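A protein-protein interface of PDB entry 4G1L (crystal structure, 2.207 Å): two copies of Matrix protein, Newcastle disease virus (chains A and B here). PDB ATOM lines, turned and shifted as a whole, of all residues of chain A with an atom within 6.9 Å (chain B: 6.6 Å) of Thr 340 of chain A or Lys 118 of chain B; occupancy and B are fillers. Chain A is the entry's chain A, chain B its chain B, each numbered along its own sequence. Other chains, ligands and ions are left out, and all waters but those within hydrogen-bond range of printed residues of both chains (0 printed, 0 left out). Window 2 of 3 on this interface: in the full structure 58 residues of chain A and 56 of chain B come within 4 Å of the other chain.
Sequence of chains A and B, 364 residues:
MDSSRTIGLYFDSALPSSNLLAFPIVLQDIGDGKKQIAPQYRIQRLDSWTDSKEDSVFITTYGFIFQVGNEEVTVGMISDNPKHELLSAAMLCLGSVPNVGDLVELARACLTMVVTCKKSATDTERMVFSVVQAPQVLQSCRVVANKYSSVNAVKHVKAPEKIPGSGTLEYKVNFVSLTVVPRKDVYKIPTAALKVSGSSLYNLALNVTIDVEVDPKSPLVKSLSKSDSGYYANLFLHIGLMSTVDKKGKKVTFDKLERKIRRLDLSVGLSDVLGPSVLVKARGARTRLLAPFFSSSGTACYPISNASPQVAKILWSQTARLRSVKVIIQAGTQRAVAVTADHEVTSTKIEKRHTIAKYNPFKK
Printed residues of chain B within 4 Å of Gln 330 of chain A: Lys 119 (3.2 Å) and Ser 120 (2.9 Å). Of the printed residues of chain B, Ala 338 of chain A touches Val 128 and Ser 130. Val 339 of chain A touches none of the printed residues of chain B. Thr 340 of chain A touches just one residue of chain B: Lys 118 (3.0 Å). Printed residues of chain B within 4 Å of Asp 342 of chain A: Lys 118. Lys 118 of chain B touches just these residues of chain A: Val 337, Thr 340 and Asp 342. Of the printed residues of chain A, Ser 130 of chain B touches Ala 338.
O of Ser 120 of chain B is in hydrogen-bond range of N of Arg 126 of chain B. O of Lys 118 of chain B sits at hydrogen-bond distance from N of Val 128 of chain B (2.9 Å). NZ of Lys 119 of chain B lies within hydrogen-bond range of O of Ile 163 of chain B (3.0 Å). The side-chain hydroxyl of Thr 340 of chain A lies close to the backbone carbonyl oxygen of Ala 336 of chain A. The side-chain carboxylate (OD2) of Asp 342 of chain A sits at hydrogen-bond distance from the side-chain amide nitrogen (NE2) of Gln 330 of chain A (2.9 Å). The backbone carbonyl oxygen of Thr 116 of chain B is in hydrogen-bond range of the backbone NH of Ser 130 of chain B (2.7 Å).
Of the 15 printed residues of chain A, 5 touch a printed residue of chain B. Hydrophobic or aromatic side chains of chain A within 4 Å of the printed part of chain B: Val 337 and Ala 338. Hydrophobic or aromatic side chains of chain B that line the printed part of chain A: Val 128. Among the printed residues, 7 pairs touch across the chains. Among the printed residues, Asp or Glu carboxylates within 4 Å of a Lys or Arg side-chain nitrogen of the other chain: Asp 342 of chain A with Lys 118 of chain B (3.1 Å).
No position is printed for both chains.
Among the printed residues, pairs that only touch across the chains: Ala 338 of chain A with Val 128 of chain B.
The side-chain amide nitrogen of Gln 330 of chain A sits at hydrogen-bond distance from the backbone carbonyl oxygen of Lys 119 of chain B. The backbone carbonyl oxygen of Ala 338 of chain A lies within hydrogen-bond range of the side-chain hydroxyl of Ser 130 of chain B, at 2.6 Å. NZ of Lys 118 of chain B lies within hydrogen-bond range of O of Thr 340 of chain A. OE1 of Gln 330 of chain A is in hydrogen-bond range of OG of Ser 120 of chain B, at 2.9 Å. O of Val 337 of chain A is in hydrogen-bond range of NZ of Lys 118 of chain B (3.0 Å). OD1 of Asp 342 of chain A is in salt-bridge range of NZ of Lys 118 of chain B (3.1 Å).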
ATOM      1  N   TYR A 202      26.186   9.804   3.350  1.00  0.00           N
ATOM      2  CA  TYR A 202      27.124  10.349   4.338  1.00  0.00           C
ATOM      3  C   TYR A 202      28.336  10.807   3.627  1.00  0.00           C
ATOM      4  O   TYR A 202      28.709  10.278   2.583  1.00  0.00           O
ATOM      5  CB  TYR A 202      27.594   9.325   5.342  1.00  0.00           C
ATOM      6  CG  TYR A 202      26.537   8.819   6.258  1.00  0.00           C
ATOM      7  CD1 TYR A 202      26.059   9.600   7.303  1.00  0.00           C
ATOM      8  CD2 TYR A 202      26.048   7.528   6.108  1.00  0.00           C
ATOM      9  CE1 TYR A 202      25.102   9.105   8.181  1.00  0.00           C
ATOM     10  CE2 TYR A 202      25.111   7.013   6.975  1.00  0.00           C
ATOM     11  CZ  TYR A 202      24.627   7.804   8.001  1.00  0.00           C
ATOM     12  OH  TYR A 202      23.678   7.284   8.839  1.00  0.00           O
ATOM     13  N   ILE A 329      32.666  10.613   9.855  1.00  0.00           N
ATOM     14  CA  ILE A 329      31.432  10.487   9.072  1.00  0.00           C
ATOM     15  C   ILE A 329      30.580  11.645   9.535  1.00  0.00           C
ATOM     16  O   ILE A 329      30.532  11.889  10.745  1.00  0.00           O
ATOM     17  CB  ILE A 329      30.644   9.186   9.395  1.00  0.00           C
ATOM     18  CG1 ILE A 329      31.344   7.937   8.823  1.00  0.00           C
ATOM     19  CG2 ILE A 329      29.245   9.238   8.846  1.00  0.00           C
ATOM     20  CD1 ILE A 329      32.144   7.208   9.880  1.00  0.00           C
ATOM     21  N   GLN A 330      29.950  12.336   8.580  1.00  0.00           N
ATOM     22  CA  GLN A 330      29.100  13.494   8.789  1.00  0.00           C
ATOM     23  C   GLN A 330      27.899  13.285   7.914  1.00  0.00           C
ATOM     24  O   GLN A 330      27.948  12.444   7.034  1.00  0.00           O
ATOM     25  CB  GLN A 330      29.776  14.793   8.316  1.00  0.00           C
ATOM     26  CG  GLN A 330      31.181  15.087   8.877  1.00  0.00           C
ATOM     27  CD  GLN A 330      31.567  16.539   8.587  1.00  0.00           C
ATOM     28  OE1 GLN A 330      31.596  16.963   7.423  1.00  0.00           O
ATOM     29  NE2 GLN A 330      31.825  17.313   9.642  1.00  0.00           N
ATOM     30  N   ALA A 331      26.848  14.072   8.125  1.00  0.00           N
ATOM     31  CA  ALA A 331      25.675  13.985   7.255  1.00  0.00           C
ATOM     32  C   ALA A 331      26.084  14.438   5.876  1.00  0.00           C
ATOM     33  O   ALA A 331      27.122  15.085   5.715  1.00  0.00           O
ATOM     34  CB  ALA A 331      24.548  14.856   7.768  1.00  0.00           C
ATOM     35  N   GLY A 332      25.260  14.123   4.900  1.00  0.00           N
ATOM     36  CA  GLY A 332      25.598  14.326   3.495  1.00  0.00           C
ATOM     37  C   GLY A 332      25.053  15.563   2.839  1.00  0.00           C
ATOM     38  O   GLY A 332      25.007  15.647   1.647  1.00  0.00           O
ATOM     39  N   THR A 333      24.571  16.487   3.623  1.00  0.00           N
ATOM     40  CA  THR A 333      24.242  17.847   3.134  1.00  0.00           C
ATOM     41  C   THR A 333      24.753  18.770   4.246  1.00  0.00           C
ATOM     42  O   THR A 333      24.663  18.414   5.430  1.00  0.00           O
ATOM     43  CB  THR A 333      22.724  18.133   2.885  1.00  0.00           C
ATOM     44  OG1 THR A 333      21.983  18.133   4.115  1.00  0.00           O
ATOM     45  CG2 THR A 333      22.098  17.132   1.944  1.00  0.00           C
ATOM     46  N   ARG A 335      23.471  21.447   5.331  1.00  0.00           N
ATOM     47  CA  ARG A 335      22.310  21.766   6.184  1.00  0.00           C
ATOM     48  C   ARG A 335      22.247  20.773   7.344  1.00  0.00           C
ATOM     49  O   ARG A 335      22.217  21.182   8.520  1.00  0.00           O
ATOM     50  CB  ARG A 335      21.028  21.759   5.371  1.00  0.00           C
ATOM     51  CG  ARG A 335      19.764  21.891   6.217  1.00  0.00           C
ATOM     52  CD  ARG A 335      18.503  21.834   5.353  1.00  0.00           C
ATOM     53  NE  ARG A 335      18.164  23.168   4.850  1.00  0.00           N
ATOM     54  CZ  ARG A 335      18.545  23.665   3.672  1.00  0.00           C
ATOM     55  NH1 ARG A 335      19.270  22.925   2.826  1.00  0.00           N
ATOM     56  NH2 ARG A 335      18.195  24.910   3.345  1.00  0.00           N
ATOM     57  N   ALA A 336      22.328  19.474   7.013  1.00  0.00           N
ATOM     58  CA  ALA A 336      22.345  18.432   8.031  1.00  0.00           C
ATOM     59  C   ALA A 336      23.644  18.391   8.808  1.00  0.00           C
ATOM     60  O   ALA A 336      23.618  18.135  10.031  1.00  0.00           O
ATOM     61  CB  ALA A 336      21.979  17.060   7.455  1.00  0.00           C
ATOM     62  N   VAL A 337      24.783  18.673   8.164  1.00  0.00           N
ATOM     63  CA  VAL A 337      26.037  18.732   8.977  1.00  0.00           C
ATOM     64  C   VAL A 337      25.835  19.713  10.136  1.00  0.00           C
ATOM     65  O   VAL A 337      26.232  19.447  11.267  1.00  0.00           O
ATOM     66  CB  VAL A 337      27.317  19.090   8.182  1.00  0.00           C
ATOM     67  CG1 VAL A 337      28.499  19.339   9.108  1.00  0.00           C
ATOM     68  CG2 VAL A 337      27.667  18.012   7.173  1.00  0.00           C
ATOM     69  N   ALA A 338      25.182  20.833   9.857  1.00  0.00           N
ATOM     70  CA  ALA A 338      24.942  21.834  10.894  1.00  0.00           C
ATOM     71  C   ALA A 338      24.172  21.335  12.126  1.00  0.00           C
ATOM     72  O   ALA A 338      24.453  21.775  13.259  1.00  0.00           O
ATOM     73  CB  ALA A 338      24.245  23.049  10.322  1.00  0.00           C
ATOM     74  N   VAL A 339      23.197  20.460  11.918  1.00  0.00           N
ATOM     75  CA  VAL A 339      22.407  20.037  13.050  1.00  0.00           C
ATOM     76  C   VAL A 339      22.766  18.638  13.552  1.00  0.00           C
ATOM     77  O   VAL A 339      22.219  18.212  14.558  1.00  0.00           O
ATOM     78  CB  VAL A 339      20.902  20.126  12.766  1.00  0.00           C
ATOM     79  CG1 VAL A 339      20.497  21.576  12.527  1.00  0.00           C
ATOM     80  CG2 VAL A 339      20.505  19.253  11.572  1.00  0.00           C
ATOM     81  N   THR A 340      23.669  17.914  12.874  1.00  0.00           N
ATOM     82  CA  THR A 340      23.945  16.531  13.287  1.00  0.00           C
ATOM     83  C   THR A 340      25.396  16.310  13.679  1.00  0.00           C
ATOM     84  O   THR A 340      26.320  16.669  12.917  1.00  0.00           O
ATOM     85  CB  THR A 340      23.477  15.444  12.264  1.00  0.00           C
ATOM     86  OG1 THR A 340      24.483  15.212  11.276  1.00  0.00           O
ATOM     87  CG2 THR A 340      22.142  15.800  11.578  1.00  0.00           C
ATOM     88  N   ALA A 341      25.599  15.717  14.859  1.00  0.00           N
ATOM     89  CA  ALA A 341      26.948  15.534  15.384  1.00  0.00           C
ATOM     90  C   ALA A 341      27.730  14.492  14.559  1.00  0.00           C
ATOM     91  O   ALA A 341      27.160  13.511  14.055  1.00  0.00           O
ATOM     92  CB  ALA A 341      26.937  15.181  16.875  1.00  0.00           C
ATOM     93  N   ASP A 342      29.033  14.715  14.431  1.00  0.00           N
ATOM     94  CA  ASP A 342      29.897  13.848  13.635  1.00  0.00           C
ATOM     95  C   ASP A 342      30.177  12.536  14.345  1.00  0.00           C
ATOM     96  O   ASP A 342      30.112  12.476  15.570  1.00  0.00           O
ATOM     97  CB  ASP A 342      31.195  14.577  13.330  1.00  0.00           C
ATOM     98  CG  ASP A 342      30.974  15.831  12.460  1.00  0.00           C
ATOM     99  OD1 ASP A 342      29.887  15.967  11.816  1.00  0.00           O
ATOM    100  OD2 ASP A 342      31.905  16.669  12.426  1.00  0.00           O
ATOM    101  N   HIS A 343      30.462  11.487  13.572  1.00  0.00           N
ATOM    102  CA  HIS A 343      30.848  10.207  14.147  1.00  0.00           C
ATOM    103  C   HIS A 343      32.282   9.934  13.834  1.00  0.00           C
ATOM    104  O   HIS A 343      32.659   9.760  12.654  1.00  0.00           O
ATOM    105  CB  HIS A 343      29.963   9.081  13.612  1.00  0.00           C
ATOM    106  CG  HIS A 343      30.189   7.746  14.298  1.00  0.00           C
ATOM    107  ND1 HIS A 343      29.448   7.333  15.350  1.00  0.00           N
ATOM    108  CD2 HIS A 343      31.114   6.727  14.046  1.00  0.00           C
ATOM    109  CE1 HIS A 343      29.875   6.119  15.749  1.00  0.00           C
ATOM    110  NE2 HIS A 343      30.895   5.750  14.947  1.00  0.00           N
ATOM    111  N   THR B 116      27.226  28.146  17.045  1.00  0.00           N
ATOM    112  CA  THR B 116      28.306  27.173  17.089  1.00  0.00           C
ATOM    113  C   THR B 116      28.854  26.909  15.686  1.00  0.00           C
ATOM    114  O   THR B 116      28.246  27.253  14.675  1.00  0.00           O
ATOM    115  CB  THR B 116      27.923  25.847  17.799  1.00  0.00           C
ATOM    116  OG1 THR B 116      26.941  25.145  17.033  1.00  0.00           O
ATOM    117  CG2 THR B 116      27.365  26.118  19.180  1.00  0.00           C
ATOM    118  N   CYS B 117      30.020  26.317  15.619  1.00  0.00           N
ATOM    119  CA  CYS B 117      30.566  26.026  14.316  1.00  0.00           C
ATOM    120  C   CYS B 117      31.367  24.767  14.433  1.00  0.00           C
ATOM    121  O   CYS B 117      31.606  24.273  15.532  1.00  0.00           O
ATOM    122  CB  CYS B 117      31.412  27.195  13.790  1.00  0.00           C
ATOM    123  SG  CYS B 117      32.596  27.822  14.987  1.00  0.00           S
ATOM    124  N   LYS B 118      31.732  24.223  13.280  1.00  0.00           N
ATOM    125  CA  LYS B 118      32.526  23.016  13.194  1.00  0.00           C
ATOM    126  C   LYS B 118      33.032  23.023  11.756  1.00  0.00           C
ATOM    127  O   LYS B 118      32.466  23.725  10.905  1.00  0.00           O
ATOM    128  CB  LYS B 118      31.647  21.795  13.474  1.00  0.00           C
ATOM    129  CG  LYS B 118      30.545  21.625  12.437  1.00  0.00           C
ATOM    130  CD  LYS B 118      29.341  20.908  13.013  1.00  0.00           C
ATOM    131  CE  LYS B 118      29.658  19.468  13.382  1.00  0.00           C
ATOM    132  NZ  LYS B 118      28.560  18.598  12.875  1.00  0.00           N
ATOM    133  N   LYS B 119      34.117  22.298  11.496  1.00  0.00           N
ATOM    134  CA  LYS B 119      34.663  22.167  10.159  1.00  0.00           C
ATOM    135  C   LYS B 119      33.875  21.122   9.375  1.00  0.00           C
ATOM    136  O   LYS B 119      33.447  20.086   9.903  1.00  0.00           O
ATOM    137  CB  LYS B 119      36.133  21.754  10.202  1.00  0.00           C
ATOM    138  CG  LYS B 119      37.111  22.859  10.513  1.00  0.00           C
ATOM    139  CD  LYS B 119      38.201  22.941   9.455  1.00  0.00           C
ATOM    140  CE  LYS B 119      39.565  22.525  10.003  1.00  0.00           C
ATOM    141  NZ  LYS B 119      40.507  23.676  10.148  1.00  0.00           N
ATOM    142  N   SER B 120      33.775  21.315   8.085  1.00  0.00           N
ATOM    143  CA  SER B 120      33.278  20.292   7.206  1.00  0.00           C
ATOM    144  C   SER B 120      34.051  20.428   5.936  1.00  0.00           C
ATOM    145  O   SER B 120      34.971  21.189   5.885  1.00  0.00           O
ATOM    146  CB  SER B 120      31.803  20.435   6.977  1.00  0.00           C
ATOM    147  OG  SER B 120      31.369  19.512   6.035  1.00  0.00           O
ATOM    148  N   ARG B 126      35.297  23.660   4.701  1.00  0.00           N
ATOM    149  CA  ARG B 126      34.156  24.524   4.974  1.00  0.00           C
ATOM    150  C   ARG B 126      34.071  24.836   6.428  1.00  0.00           C
ATOM    151  O   ARG B 126      34.417  24.023   7.268  1.00  0.00           O
ATOM    152  CB  ARG B 126      32.834  23.955   4.400  1.00  0.00           C
ATOM    153  CG  ARG B 126      32.806  24.236   2.913  1.00  0.00           C
ATOM    154  CD  ARG B 126      31.540  23.899   2.171  1.00  0.00           C
ATOM    155  NE  ARG B 126      30.742  25.098   1.983  1.00  0.00           N
ATOM    156  CZ  ARG B 126      30.972  26.039   1.080  1.00  0.00           C
ATOM    157  NH1 ARG B 126      31.990  25.919   0.234  1.00  0.00           N
ATOM    158  NH2 ARG B 126      30.176  27.115   1.039  1.00  0.00           N
ATOM    159  N   MET B 127      33.691  26.056   6.742  1.00  0.00           N
ATOM    160  CA  MET B 127      33.252  26.305   8.116  1.00  0.00           C
ATOM    161  C   MET B 127      31.733  26.296   8.103  1.00  0.00           C
ATOM    162  O   MET B 127      31.128  26.955   7.267  1.00  0.00           O
ATOM    163  CB  MET B 127      33.767  27.626   8.637  1.00  0.00           C
ATOM    164  CG  MET B 127      33.862  27.601  10.124  1.00  0.00           C
ATOM    165  SD  MET B 127      35.124  26.433  10.681  1.00  0.00           S
ATOM    166  CE  MET B 127      34.674  26.437  12.407  1.00  0.00           C
ATOM    167  N   VAL B 128      31.130  25.551   9.020  1.00  0.00           N
ATOM    168  CA  VAL B 128      29.659  25.484   9.104  1.00  0.00           C
ATOM    169  C   VAL B 128      29.276  26.164  10.389  1.00  0.00           C
ATOM    170  O   VAL B 128      29.657  25.730  11.473  1.00  0.00           O
ATOM    171  CB  VAL B 128      29.137  24.023   9.054  1.00  0.00           C
ATOM    172  CG1 VAL B 128      27.606  23.957   9.083  1.00  0.00           C
ATOM    173  CG2 VAL B 128      29.719  23.306   7.846  1.00  0.00           C
ATOM    174  N   PHE B 129      28.566  27.273  10.269  1.00  0.00           N
ATOM    175  CA  PHE B 129      28.024  27.952  11.448  1.00  0.00           C
ATOM    176  C   PHE B 129      26.575  27.561  11.602  1.00  0.00           C
ATOM    177  O   PHE B 129      25.784  27.634  10.636  1.00  0.00           O
ATOM    178  CB  PHE B 129      28.099  29.473  11.323  1.00  0.00           C
ATOM    179  CG  PHE B 129      29.485  30.008  11.221  1.00  0.00           C
ATOM    180  CD1 PHE B 129      30.185  29.954  10.003  1.00  0.00           C
ATOM    181  CD2 PHE B 129      30.100  30.576  12.331  1.00  0.00           C
ATOM    182  CE1 PHE B 129      31.478  30.475   9.908  1.00  0.00           C
ATOM    183  CE2 PHE B 129      31.402  31.074  12.249  1.00  0.00           C
ATOM    184  CZ  PHE B 129      32.089  31.013  11.026  1.00  0.00           C
ATOM    185  N   SER B 130      26.240  27.169  12.825  1.00  0.00           N
ATOM    186  CA  SER B 130      24.899  26.780  13.195  1.00  0.00           C
ATOM    187  C   SER B 130      24.346  27.833  14.130  1.00  0.00           C
ATOM    188  O   SER B 130      24.854  28.032  15.241  1.00  0.00           O
ATOM    189  CB  SER B 130      24.914  25.444  13.931  1.00  0.00           C
ATOM    190  OG  SER B 130      24.901  24.358  13.037  1.00  0.00           O
ATOM    191  N   ILE B 163      42.090  25.527  13.551  1.00  0.00           N
ATOM    192  CA  ILE B 163      40.800  25.037  14.023  1.00  0.00           C
ATOM    193  C   ILE B 163      40.756  23.517  14.019  1.00  0.00           C
ATOM    194  O   ILE B 163      40.919  22.932  12.979  1.00  0.00           O
ATOM    195  CB  ILE B 163      39.669  25.495  13.083  1.00  0.00           C
ATOM    196  CG1 ILE B 163      39.757  27.013  12.857  1.00  0.00           C
ATOM    197  CG2 ILE B 163      38.285  25.054  13.605  1.00  0.00           C
ATOM    198  CD1 ILE B 163      39.061  27.405  11.572  1.00  0.00           C
ATOM    199  N   PRO B 164      40.466  22.883  15.167  1.00  0.00           N
ATOM    200  CA  PRO B 164      40.424  21.409  15.152  1.00  0.00           C
ATOM    201  C   PRO B 164      39.182  20.880  14.426  1.00  0.00           C
ATOM    202  O   PRO B 164      38.172  21.500  14.470  1.00  0.00           O
ATOM    203  CB  PRO B 164      40.376  21.054  16.636  1.00  0.00           C
ATOM    204  CG  PRO B 164      39.649  22.222  17.270  1.00  0.00           C
ATOM    205  CD  PRO B 164      40.140  23.438  16.500  1.00  0.00           C
ATOM    206  N   GLY B 165      39.269  19.749  13.759  1.00  0.00           N
ATOM    207  CA  GLY B 165      38.160  19.267  12.943  1.00  0.00           C
ATOM    208  C   GLY B 165      37.223  18.412  13.773  1.00  0.00           C
ATOM    209  O   GLY B 165      36.407  17.697  13.240  1.00  0.00           O
ATOM    210  N   GLY B 167      35.689  18.510  18.237  1.00  0.00           N
ATOM    211  CA  GLY B 167      35.704  19.313  19.447  1.00  0.00           C
ATOM    212  C   GLY B 167      34.559  20.297  19.477  1.00  0.00           C
ATOM    213  O   GLY B 167      33.796  20.419  18.504  1.00  0.00           O
ATOM    214  N   LEU B 169      33.143  23.928  19.683  1.00  0.00           N
ATOM    215  CA  LEU B 169      33.466  25.291  19.216  1.00  0.00           C
ATOM    216  C   LEU B 169      32.271  26.225  19.038  1.00  0.00           C
ATOM    217  O   LEU B 169      31.177  25.851  18.566  1.00  0.00           O
ATOM    218  CB  LEU B 169      34.228  25.273  17.888  1.00  0.00           C
ATOM    219  CG  LEU B 169      35.361  24.307  17.578  1.00  0.00           C
ATOM    220  CD1 LEU B 169      35.777  24.532  16.121  1.00  0.00           C
ATOM    221  CD2 LEU B 169      36.567  24.438  18.498  1.00  0.00           C
